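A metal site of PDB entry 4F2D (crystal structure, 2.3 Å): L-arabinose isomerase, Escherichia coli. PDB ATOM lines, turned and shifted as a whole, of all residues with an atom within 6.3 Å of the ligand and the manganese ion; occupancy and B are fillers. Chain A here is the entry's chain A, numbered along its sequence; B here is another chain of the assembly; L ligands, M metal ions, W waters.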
ATOM      1  N   MET A 185       6.018  -2.914  30.111  1.00  0.00           N
ATOM      2  CA  MET A 185       6.979  -2.241  29.242  1.00  0.00           C
ATOM      3  C   MET A 185       6.730  -0.765  29.385  1.00  0.00           C
ATOM      4  O   MET A 185       5.569  -0.313  29.354  1.00  0.00           O
ATOM      5  CB  MET A 185       6.807  -2.639  27.771  1.00  0.00           C
ATOM      6  CG  MET A 185       7.823  -1.989  26.829  1.00  0.00           C
ATOM      7  SD  MET A 185       7.513  -2.498  24.928  1.00  0.00           S
ATOM      8  CE  MET A 185       6.924  -4.361  25.071  1.00  0.00           C
ATOM      9  N   PHE A 279      10.885  -8.004  29.037  1.00  0.00           N
ATOM     10  CA  PHE A 279      12.264  -8.039  28.534  1.00  0.00           C
ATOM     11  C   PHE A 279      13.121  -6.877  29.056  1.00  0.00           C
ATOM     12  O   PHE A 279      14.342  -6.923  28.945  1.00  0.00           O
ATOM     13  CB  PHE A 279      12.311  -8.108  27.005  1.00  0.00           C
ATOM     14  CG  PHE A 279      11.680  -6.938  26.302  1.00  0.00           C
ATOM     15  CD1 PHE A 279      12.316  -5.703  26.256  1.00  0.00           C
ATOM     16  CD2 PHE A 279      10.446  -7.084  25.669  1.00  0.00           C
ATOM     17  CE1 PHE A 279      11.727  -4.629  25.605  1.00  0.00           C
ATOM     18  CE2 PHE A 279       9.862  -6.019  25.015  1.00  0.00           C
ATOM     19  CZ  PHE A 279      10.494  -4.789  24.982  1.00  0.00           C
ATOM     20  N   GLY A 305       3.113 -11.201  26.992  1.00  0.00           N
ATOM     21  CA  GLY A 305       4.426 -10.568  27.064  1.00  0.00           C
ATOM     22  C   GLY A 305       4.380  -9.176  27.671  1.00  0.00           C
ATOM     23  O   GLY A 305       3.297  -8.613  27.888  1.00  0.00           O
ATOM     24  N   GLU A 306       5.558  -8.633  27.930  1.00  0.00           N
ATOM     25  CA  GLU A 306       5.760  -7.290  28.499  1.00  0.00           C
ATOM     26  C   GLU A 306       4.742  -6.859  29.572  1.00  0.00           C
ATOM     27  O   GLU A 306       4.172  -5.778  29.528  1.00  0.00           O
ATOM     28  CB  GLU A 306       5.866  -6.240  27.386  1.00  0.00           C
ATOM     29  CG  GLU A 306       4.821  -6.331  26.292  1.00  0.00           C
ATOM     30  CD  GLU A 306       5.299  -7.082  25.057  1.00  0.00           C
ATOM     31  OE1 GLU A 306       4.774  -6.804  23.959  1.00  0.00           O
ATOM     32  OE2 GLU A 306       6.189  -7.932  25.190  1.00  0.00           O
ATOM     33  N   PHE A 331      -1.456 -17.254  23.098  1.00  0.00           N
ATOM     34  CA  PHE A 331      -1.060 -15.857  23.059  1.00  0.00           C
ATOM     35  C   PHE A 331      -0.631 -15.535  21.630  1.00  0.00           C
ATOM     36  O   PHE A 331      -0.030 -16.381  20.967  1.00  0.00           O
ATOM     37  CB  PHE A 331       0.086 -15.594  24.022  1.00  0.00           C
ATOM     38  CG  PHE A 331       0.633 -14.192  23.964  1.00  0.00           C
ATOM     39  CD1 PHE A 331      -0.205 -13.105  24.155  1.00  0.00           C
ATOM     40  CD2 PHE A 331       1.972 -13.959  23.731  1.00  0.00           C
ATOM     41  CE1 PHE A 331       0.284 -11.811  24.107  1.00  0.00           C
ATOM     42  CE2 PHE A 331       2.477 -12.670  23.687  1.00  0.00           C
ATOM     43  CZ  PHE A 331       1.626 -11.595  23.861  1.00  0.00           C
ATOM     44  N   GLU A 333       0.207 -12.081  18.631  1.00  0.00           N
ATOM     45  CA  GLU A 333       0.376 -10.674  18.280  1.00  0.00           C
ATOM     46  C   GLU A 333       0.412 -10.502  16.759  1.00  0.00           C
ATOM     47  O   GLU A 333       1.074 -11.279  16.069  1.00  0.00           O
ATOM     48  CB  GLU A 333       1.663 -10.132  18.875  1.00  0.00           C
ATOM     49  CG  GLU A 333       1.766  -8.614  18.866  1.00  0.00           C
ATOM     50  CD  GLU A 333       3.120  -8.127  19.324  1.00  0.00           C
ATOM     51  OE1 GLU A 333       3.188  -7.450  20.359  1.00  0.00           O
ATOM     52  OE2 GLU A 333       4.119  -8.419  18.650  1.00  0.00           O
ATOM     53  N   TYR A 335       1.915  -9.371  13.752  1.00  0.00           N
ATOM     54  CA  TYR A 335       3.284  -8.955  13.437  1.00  0.00           C
ATOM     55  C   TYR A 335       3.422  -8.185  12.124  1.00  0.00           C
ATOM     56  O   TYR A 335       3.944  -7.068  12.117  1.00  0.00           O
ATOM     57  CB  TYR A 335       4.251 -10.132  13.490  1.00  0.00           C
ATOM     58  CG  TYR A 335       5.264  -9.898  14.586  1.00  0.00           C
ATOM     59  CD1 TYR A 335       4.985 -10.223  15.905  1.00  0.00           C
ATOM     60  CD2 TYR A 335       6.451  -9.245  14.308  1.00  0.00           C
ATOM     61  CE1 TYR A 335       5.909  -9.970  16.913  1.00  0.00           C
ATOM     62  CE2 TYR A 335       7.383  -8.987  15.312  1.00  0.00           C
ATOM     63  CZ  TYR A 335       7.111  -9.347  16.604  1.00  0.00           C
ATOM     64  OH  TYR A 335       8.047  -9.098  17.605  1.00  0.00           O
ATOM     65  N   HIS A 350       5.028 -13.886  18.026  1.00  0.00           N
ATOM     66  CA  HIS A 350       5.620 -13.033  19.066  1.00  0.00           C
ATOM     67  C   HIS A 350       7.100 -13.277  19.105  1.00  0.00           C
ATOM     68  O   HIS A 350       7.590 -14.301  18.622  1.00  0.00           O
ATOM     69  CB  HIS A 350       4.989 -13.269  20.433  1.00  0.00           C
ATOM     70  CG  HIS A 350       5.091 -12.070  21.358  1.00  0.00           C
ATOM     71  ND1 HIS A 350       5.977 -12.006  22.373  1.00  0.00           N
ATOM     72  CD2 HIS A 350       4.381 -10.867  21.380  1.00  0.00           C
ATOM     73  CE1 HIS A 350       5.841 -10.830  23.002  1.00  0.00           C
ATOM     74  NE2 HIS A 350       4.869 -10.133  22.398  1.00  0.00           N
ATOM     75  N   MET A 351       7.818 -12.308  19.652  1.00  0.00           N
ATOM     76  CA  MET A 351       9.259 -12.401  19.899  1.00  0.00           C
ATOM     77  C   MET A 351       9.773 -13.808  20.087  1.00  0.00           C
ATOM     78  O   MET A 351      10.766 -14.219  19.465  1.00  0.00           O
ATOM     79  CB  MET A 351       9.379 -11.562  21.164  1.00  0.00           C
ATOM     80  CG  MET A 351      10.752 -11.457  21.804  1.00  0.00           C
ATOM     81  SD  MET A 351      10.615  -9.856  22.928  1.00  0.00           S
ATOM     82  CE  MET A 351       9.207 -10.465  24.147  1.00  0.00           C
ATOM     83  N   ILE A 373      16.435  -7.801  21.394  1.00  0.00           N
ATOM     84  CA  ILE A 373      15.512  -7.280  22.379  1.00  0.00           C
ATOM     85  C   ILE A 373      15.736  -7.933  23.730  1.00  0.00           C
ATOM     86  O   ILE A 373      15.688  -9.161  23.841  1.00  0.00           O
ATOM     87  CB  ILE A 373      14.042  -7.499  21.950  1.00  0.00           C
ATOM     88  CG1 ILE A 373      13.675  -6.586  20.775  1.00  0.00           C
ATOM     89  CG2 ILE A 373      13.084  -7.292  23.114  1.00  0.00           C
ATOM     90  CD1 ILE A 373      12.354  -6.929  20.140  1.00  0.00           C
ATOM     91  N   HIS A 449      -2.873  -4.823  20.502  1.00  0.00           N
ATOM     92  CA  HIS A 449      -1.990  -5.596  19.623  1.00  0.00           C
ATOM     93  C   HIS A 449      -1.814  -7.004  20.126  1.00  0.00           C
ATOM     94  O   HIS A 449      -1.566  -7.917  19.344  1.00  0.00           O
ATOM     95  CB  HIS A 449      -0.625  -4.925  19.481  1.00  0.00           C
ATOM     96  CG  HIS A 449       0.099  -4.687  20.790  1.00  0.00           C
ATOM     97  ND1 HIS A 449       1.195  -5.371  21.142  1.00  0.00           N
ATOM     98  CD2 HIS A 449      -0.163  -3.797  21.835  1.00  0.00           C
ATOM     99  CE1 HIS A 449       1.621  -4.955  22.352  1.00  0.00           C
ATOM    100  NE2 HIS A 449       0.789  -3.997  22.769  1.00  0.00           N
ATOM    101  N   HIS A 450      -1.921  -7.182  21.435  1.00  0.00           N
ATOM    102  CA  HIS A 450      -1.928  -8.518  22.034  1.00  0.00           C
ATOM    103  C   HIS A 450      -3.292  -9.095  22.001  1.00  0.00           C
ATOM    104  O   HIS A 450      -4.283  -8.405  22.280  1.00  0.00           O
ATOM    105  CB  HIS A 450      -1.456  -8.465  23.480  1.00  0.00           C
ATOM    106  CG  HIS A 450       0.011  -8.205  23.634  1.00  0.00           C
ATOM    107  ND1 HIS A 450       0.562  -7.860  24.811  1.00  0.00           N
ATOM    108  CD2 HIS A 450       1.061  -8.246  22.713  1.00  0.00           C
ATOM    109  CE1 HIS A 450       1.876  -7.694  24.655  1.00  0.00           C
ATOM    110  NE2 HIS A 450       2.182  -7.930  23.368  1.00  0.00           N
ATOM    111  N   GLN B  16      10.009   4.238  17.914  1.00  0.00           N
ATOM    112  CA  GLN B  16      10.623   4.229  19.241  1.00  0.00           C
ATOM    113  C   GLN B  16      12.160   4.054  19.088  1.00  0.00           C
ATOM    114  O   GLN B  16      12.709   4.177  17.991  1.00  0.00           O
ATOM    115  CB  GLN B  16      10.034   3.068  20.064  1.00  0.00           C
ATOM    116  CG  GLN B  16      10.293   1.688  19.474  1.00  0.00           C
ATOM    117  CD  GLN B  16       9.824   0.547  20.338  1.00  0.00           C
ATOM    118  OE1 GLN B  16       9.367   0.753  21.452  1.00  0.00           O
ATOM    119  NE2 GLN B  16       9.924  -0.667  19.826  1.00  0.00           N
ATOM    120  N   LEU B  18      13.901   1.215  20.528  1.00  0.00           N
ATOM    121  CA  LEU B  18      14.259  -0.142  20.976  1.00  0.00           C
ATOM    122  C   LEU B  18      15.327  -0.855  20.142  1.00  0.00           C
ATOM    123  O   LEU B  18      16.108  -1.642  20.680  1.00  0.00           O
ATOM    124  CB  LEU B  18      13.009  -1.017  21.059  1.00  0.00           C
ATOM    125  CG  LEU B  18      13.199  -2.348  21.795  1.00  0.00           C
ATOM    126  CD1 LEU B  18      13.752  -2.182  23.207  1.00  0.00           C
ATOM    127  CD2 LEU B  18      11.895  -3.121  21.833  1.00  0.00           C
ATOM    128  N   TYR B  19      15.365  -0.597  18.838  1.00  0.00           N
ATOM    129  CA  TYR B  19      16.292  -1.265  17.943  1.00  0.00           C
ATOM    130  C   TYR B  19      17.188  -0.314  17.146  1.00  0.00           C
ATOM    131  O   TYR B  19      18.047  -0.810  16.451  1.00  0.00           O
ATOM    132  CB  TYR B  19      15.557  -2.141  16.917  1.00  0.00           C
ATOM    133  CG  TYR B  19      14.096  -2.446  17.173  1.00  0.00           C
ATOM    134  CD1 TYR B  19      13.700  -3.614  17.842  1.00  0.00           C
ATOM    135  CD2 TYR B  19      13.102  -1.596  16.712  1.00  0.00           C
ATOM    136  CE1 TYR B  19      12.360  -3.886  18.050  1.00  0.00           C
ATOM    137  CE2 TYR B  19      11.762  -1.868  16.920  1.00  0.00           C
ATOM    138  CZ  TYR B  19      11.391  -3.013  17.589  1.00  0.00           C
ATOM    139  OH  TYR B  19      10.054  -3.257  17.786  1.00  0.00           O
ATOM    140  N   PHE B  83       6.466  -0.173  16.323  1.00  0.00           N
ATOM    141  CA  PHE B  83       5.796  -0.042  17.607  1.00  0.00           C
ATOM    142  C   PHE B  83       6.204   1.288  18.230  1.00  0.00           C
ATOM    143  O   PHE B  83       7.383   1.624  18.263  1.00  0.00           O
ATOM    144  CB  PHE B  83       6.176  -1.197  18.538  1.00  0.00           C
ATOM    145  CG  PHE B  83       5.301  -1.321  19.764  1.00  0.00           C
ATOM    146  CD1 PHE B  83       5.819  -1.143  21.038  1.00  0.00           C
ATOM    147  CD2 PHE B  83       3.958  -1.624  19.636  1.00  0.00           C
ATOM    148  CE1 PHE B  83       5.022  -1.270  22.159  1.00  0.00           C
ATOM    149  CE2 PHE B  83       3.144  -1.747  20.754  1.00  0.00           C
ATOM    150  CZ  PHE B  83       3.675  -1.573  22.021  1.00  0.00           C
ATOM    151  N   PRO B  85       5.056   3.157  21.623  1.00  0.00           N
ATOM    152  CA  PRO B  85       4.276   3.116  22.863  1.00  0.00           C
ATOM    153  C   PRO B  85       3.395   4.360  23.074  1.00  0.00           C
ATOM    154  O   PRO B  85       3.893   5.491  23.057  1.00  0.00           O
ATOM    155  CB  PRO B  85       5.340   3.007  23.936  1.00  0.00           C
ATOM    156  CG  PRO B  85       6.453   2.252  23.279  1.00  0.00           C
ATOM    157  CD  PRO B  85       6.432   2.649  21.834  1.00  0.00           C
ATOM    158  N   ASN B 122      11.196  -6.465  13.154  1.00  0.00           N
ATOM    159  CA  ASN B 122      11.440  -5.320  14.049  1.00  0.00           C
ATOM    160  C   ASN B 122      11.227  -3.955  13.361  1.00  0.00           C
ATOM    161  O   ASN B 122      10.937  -2.937  14.024  1.00  0.00           O
ATOM    162  CB  ASN B 122      12.840  -5.425  14.674  1.00  0.00           C
ATOM    163  CG  ASN B 122      12.912  -6.479  15.765  1.00  0.00           C
ATOM    164  OD1 ASN B 122      11.895  -6.939  16.271  1.00  0.00           O
ATOM    165  ND2 ASN B 122      14.128  -6.873  16.119  1.00  0.00           N
ATOM    166  N   GLN B 125       6.411  -3.210  11.472  1.00  0.00           N
ATOM    167  CA  GLN B 125       5.463  -3.772  12.453  1.00  0.00           C
ATOM    168  C   GLN B 125       4.242  -2.891  12.689  1.00  0.00           C
ATOM    169  O   GLN B 125       3.694  -2.850  13.806  1.00  0.00           O
ATOM    170  CB  GLN B 125       6.144  -4.158  13.780  1.00  0.00           C
ATOM    171  CG  GLN B 125       7.179  -3.170  14.281  1.00  0.00           C
ATOM    172  CD  GLN B 125       7.771  -3.573  15.608  1.00  0.00           C
ATOM    173  OE1 GLN B 125       7.810  -4.747  15.946  1.00  0.00           O
ATOM    174  NE2 GLN B 125       8.229  -2.587  16.365  1.00  0.00           N
ATOM    175  N   HIS B 128       0.955  -4.361  14.555  1.00  0.00           N
ATOM    176  CA  HIS B 128       0.659  -4.159  15.981  1.00  0.00           C
ATOM    177  C   HIS B 128       0.881  -2.749  16.466  1.00  0.00           C
ATOM    178  O   HIS B 128       0.144  -2.268  17.322  1.00  0.00           O
ATOM    179  CB  HIS B 128       1.373  -5.180  16.886  1.00  0.00           C
ATOM    180  CG  HIS B 128       2.864  -5.286  16.692  1.00  0.00           C
ATOM    181  ND1 HIS B 128       3.431  -6.287  16.004  1.00  0.00           N
ATOM    182  CD2 HIS B 128       3.906  -4.523  17.199  1.00  0.00           C
ATOM    183  CE1 HIS B 128       4.773  -6.149  16.033  1.00  0.00           C
ATOM    184  NE2 HIS B 128       5.054  -5.067  16.772  1.00  0.00           N
HETATM  185  C1  LIG L   1       8.755  -3.080  20.766  1.00  0.00           C
HETATM  186  O1  LIG L   1       9.056  -2.098  21.769  1.00  0.00           O
HETATM  187  C2  LIG L   1       7.957  -4.181  21.405  1.00  0.00           C
HETATM  188  O2  LIG L   1       8.733  -4.731  22.463  1.00  0.00           O
HETATM  189  C3  LIG L   1       7.604  -5.308  20.431  1.00  0.00           C
HETATM  190  O3  LIG L   1       7.183  -4.811  19.158  1.00  0.00           O
HETATM  191  C4  LIG L   1       6.505  -6.147  21.068  1.00  0.00           C
HETATM  192  O4  LIG L   1       6.344  -7.380  20.372  1.00  0.00           O
HETATM  193  C5  LIG L   1       5.163  -5.430  21.054  1.00  0.00           C
HETATM  194  O5  LIG L   1       4.286  -6.161  21.899  1.00  0.00           O
HETATM  195 MN    MN M   1       4.067  -8.111  22.379  1.00  0.00          MN
HETATM  196  O   HOH W   1       7.089  -9.703  19.764  1.00  0.00           O
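Phe 279 touches the ligand. Tyr 335 touches the ligand. Leu 18 of chain B touches the ligand (CD2 to O1, 3.0 Å). Tyr 19 of chain B touches the ligand. CD1 of Phe 83 of chain B touches O1 of the ligand (3.5 Å). Hydrophobic or aromatic side chains within 4 Å of the ligand: Met 185, Phe 279, His 449, His 450, Leu 18 of chain B, Phe 83 of chain B and His 128 of chain B. Within 4 Å of the ligand: Met 185, Phe 279, Glu 306, Glu 333, Tyr 335, His 350, His 449, His 450, Gln 16 of chain B, Leu 18 of chain B, Tyr 19 of chain B, Phe 83 of chain B, Gln 125 of chain B and His 128 of chain B. The nearest printed residue that does not touch the ligand is Ile 373 (4.8 Å).
Water W1 lies within hydrogen-bond range of OH of Tyr 335 (2.4 Å), O4 of the ligand (2.5 Å), N of Met 351 (2.7 Å) and OE2 of Glu 333 (3.4 Å).
CE1 of His 449 touches the manganese ion (3.99 Å). The nearest printed residue that does not touch the manganese ion is Phe 331 (4.5 Å).
An oxygen (O1) of the ligand sits at hydrogen-bond distance from the side-chain amide nitrogen (NE2) of Gln 16 of chain B, 2.6 Å away. A ring nitrogen (ND1) of His 449 lies close to an oxygen (O5) of the ligand, at 3.3 Å. An oxygen (O3) of the ligand sits at hydrogen-bond distance from a ring nitrogen (NE2) of His 128 of chain B (3.2 Å). The side-chain sulfur (SD) of Met 185 is in hydrogen-bond range of an oxygen (O1) of the ligand. OE1 of Gln 125 of chain B lies within hydrogen-bond range of O3 of the ligand (3.3 Å).
OH of Tyr 19 of chain B sits at hydrogen-bond distance from NE2 of Gln 125 of chain B (2.4 Å). N of Met 185 is in hydrogen-bond range of O of Glu 306, 3.5 Å away. A ring nitrogen (NE2) of His 128 of chain B is in hydrogen-bond range of the side-chain amide oxygen (OE1) of Gln 125 of chain B (2.9 Å). The side-chain amide nitrogen (NE2) of Gln 125 of chain B sits close to the backbone NH (N) of Phe 83 of chain B (3.0 Å). A ring nitrogen (ND1) of His 128 of chain B is in hydrogen-bond range of the side-chain carboxylate of Glu 333 (3.5 Å). ND1 of His 449 lies close to OE1 of Glu 333 (3.0 Å). The side-chain amide nitrogen (NE2) of Gln 16 of chain B lies within hydrogen-bond range of the side-chain hydroxyl (OH) of Tyr 19 of chain B (3.3 Å).
O5 of the ligand is bound to the manganese ion (2.0 Å). NE2 of His 450 binds the manganese ion. OE1 of Glu 306 is bound to the manganese ion (2.2 Å). The manganese ion is bound by NE2 of His 350, at 2.2 Å. OE1 of Glu 333 is bound to the manganese ion. The manganese ion has five donor atoms within binding distance.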
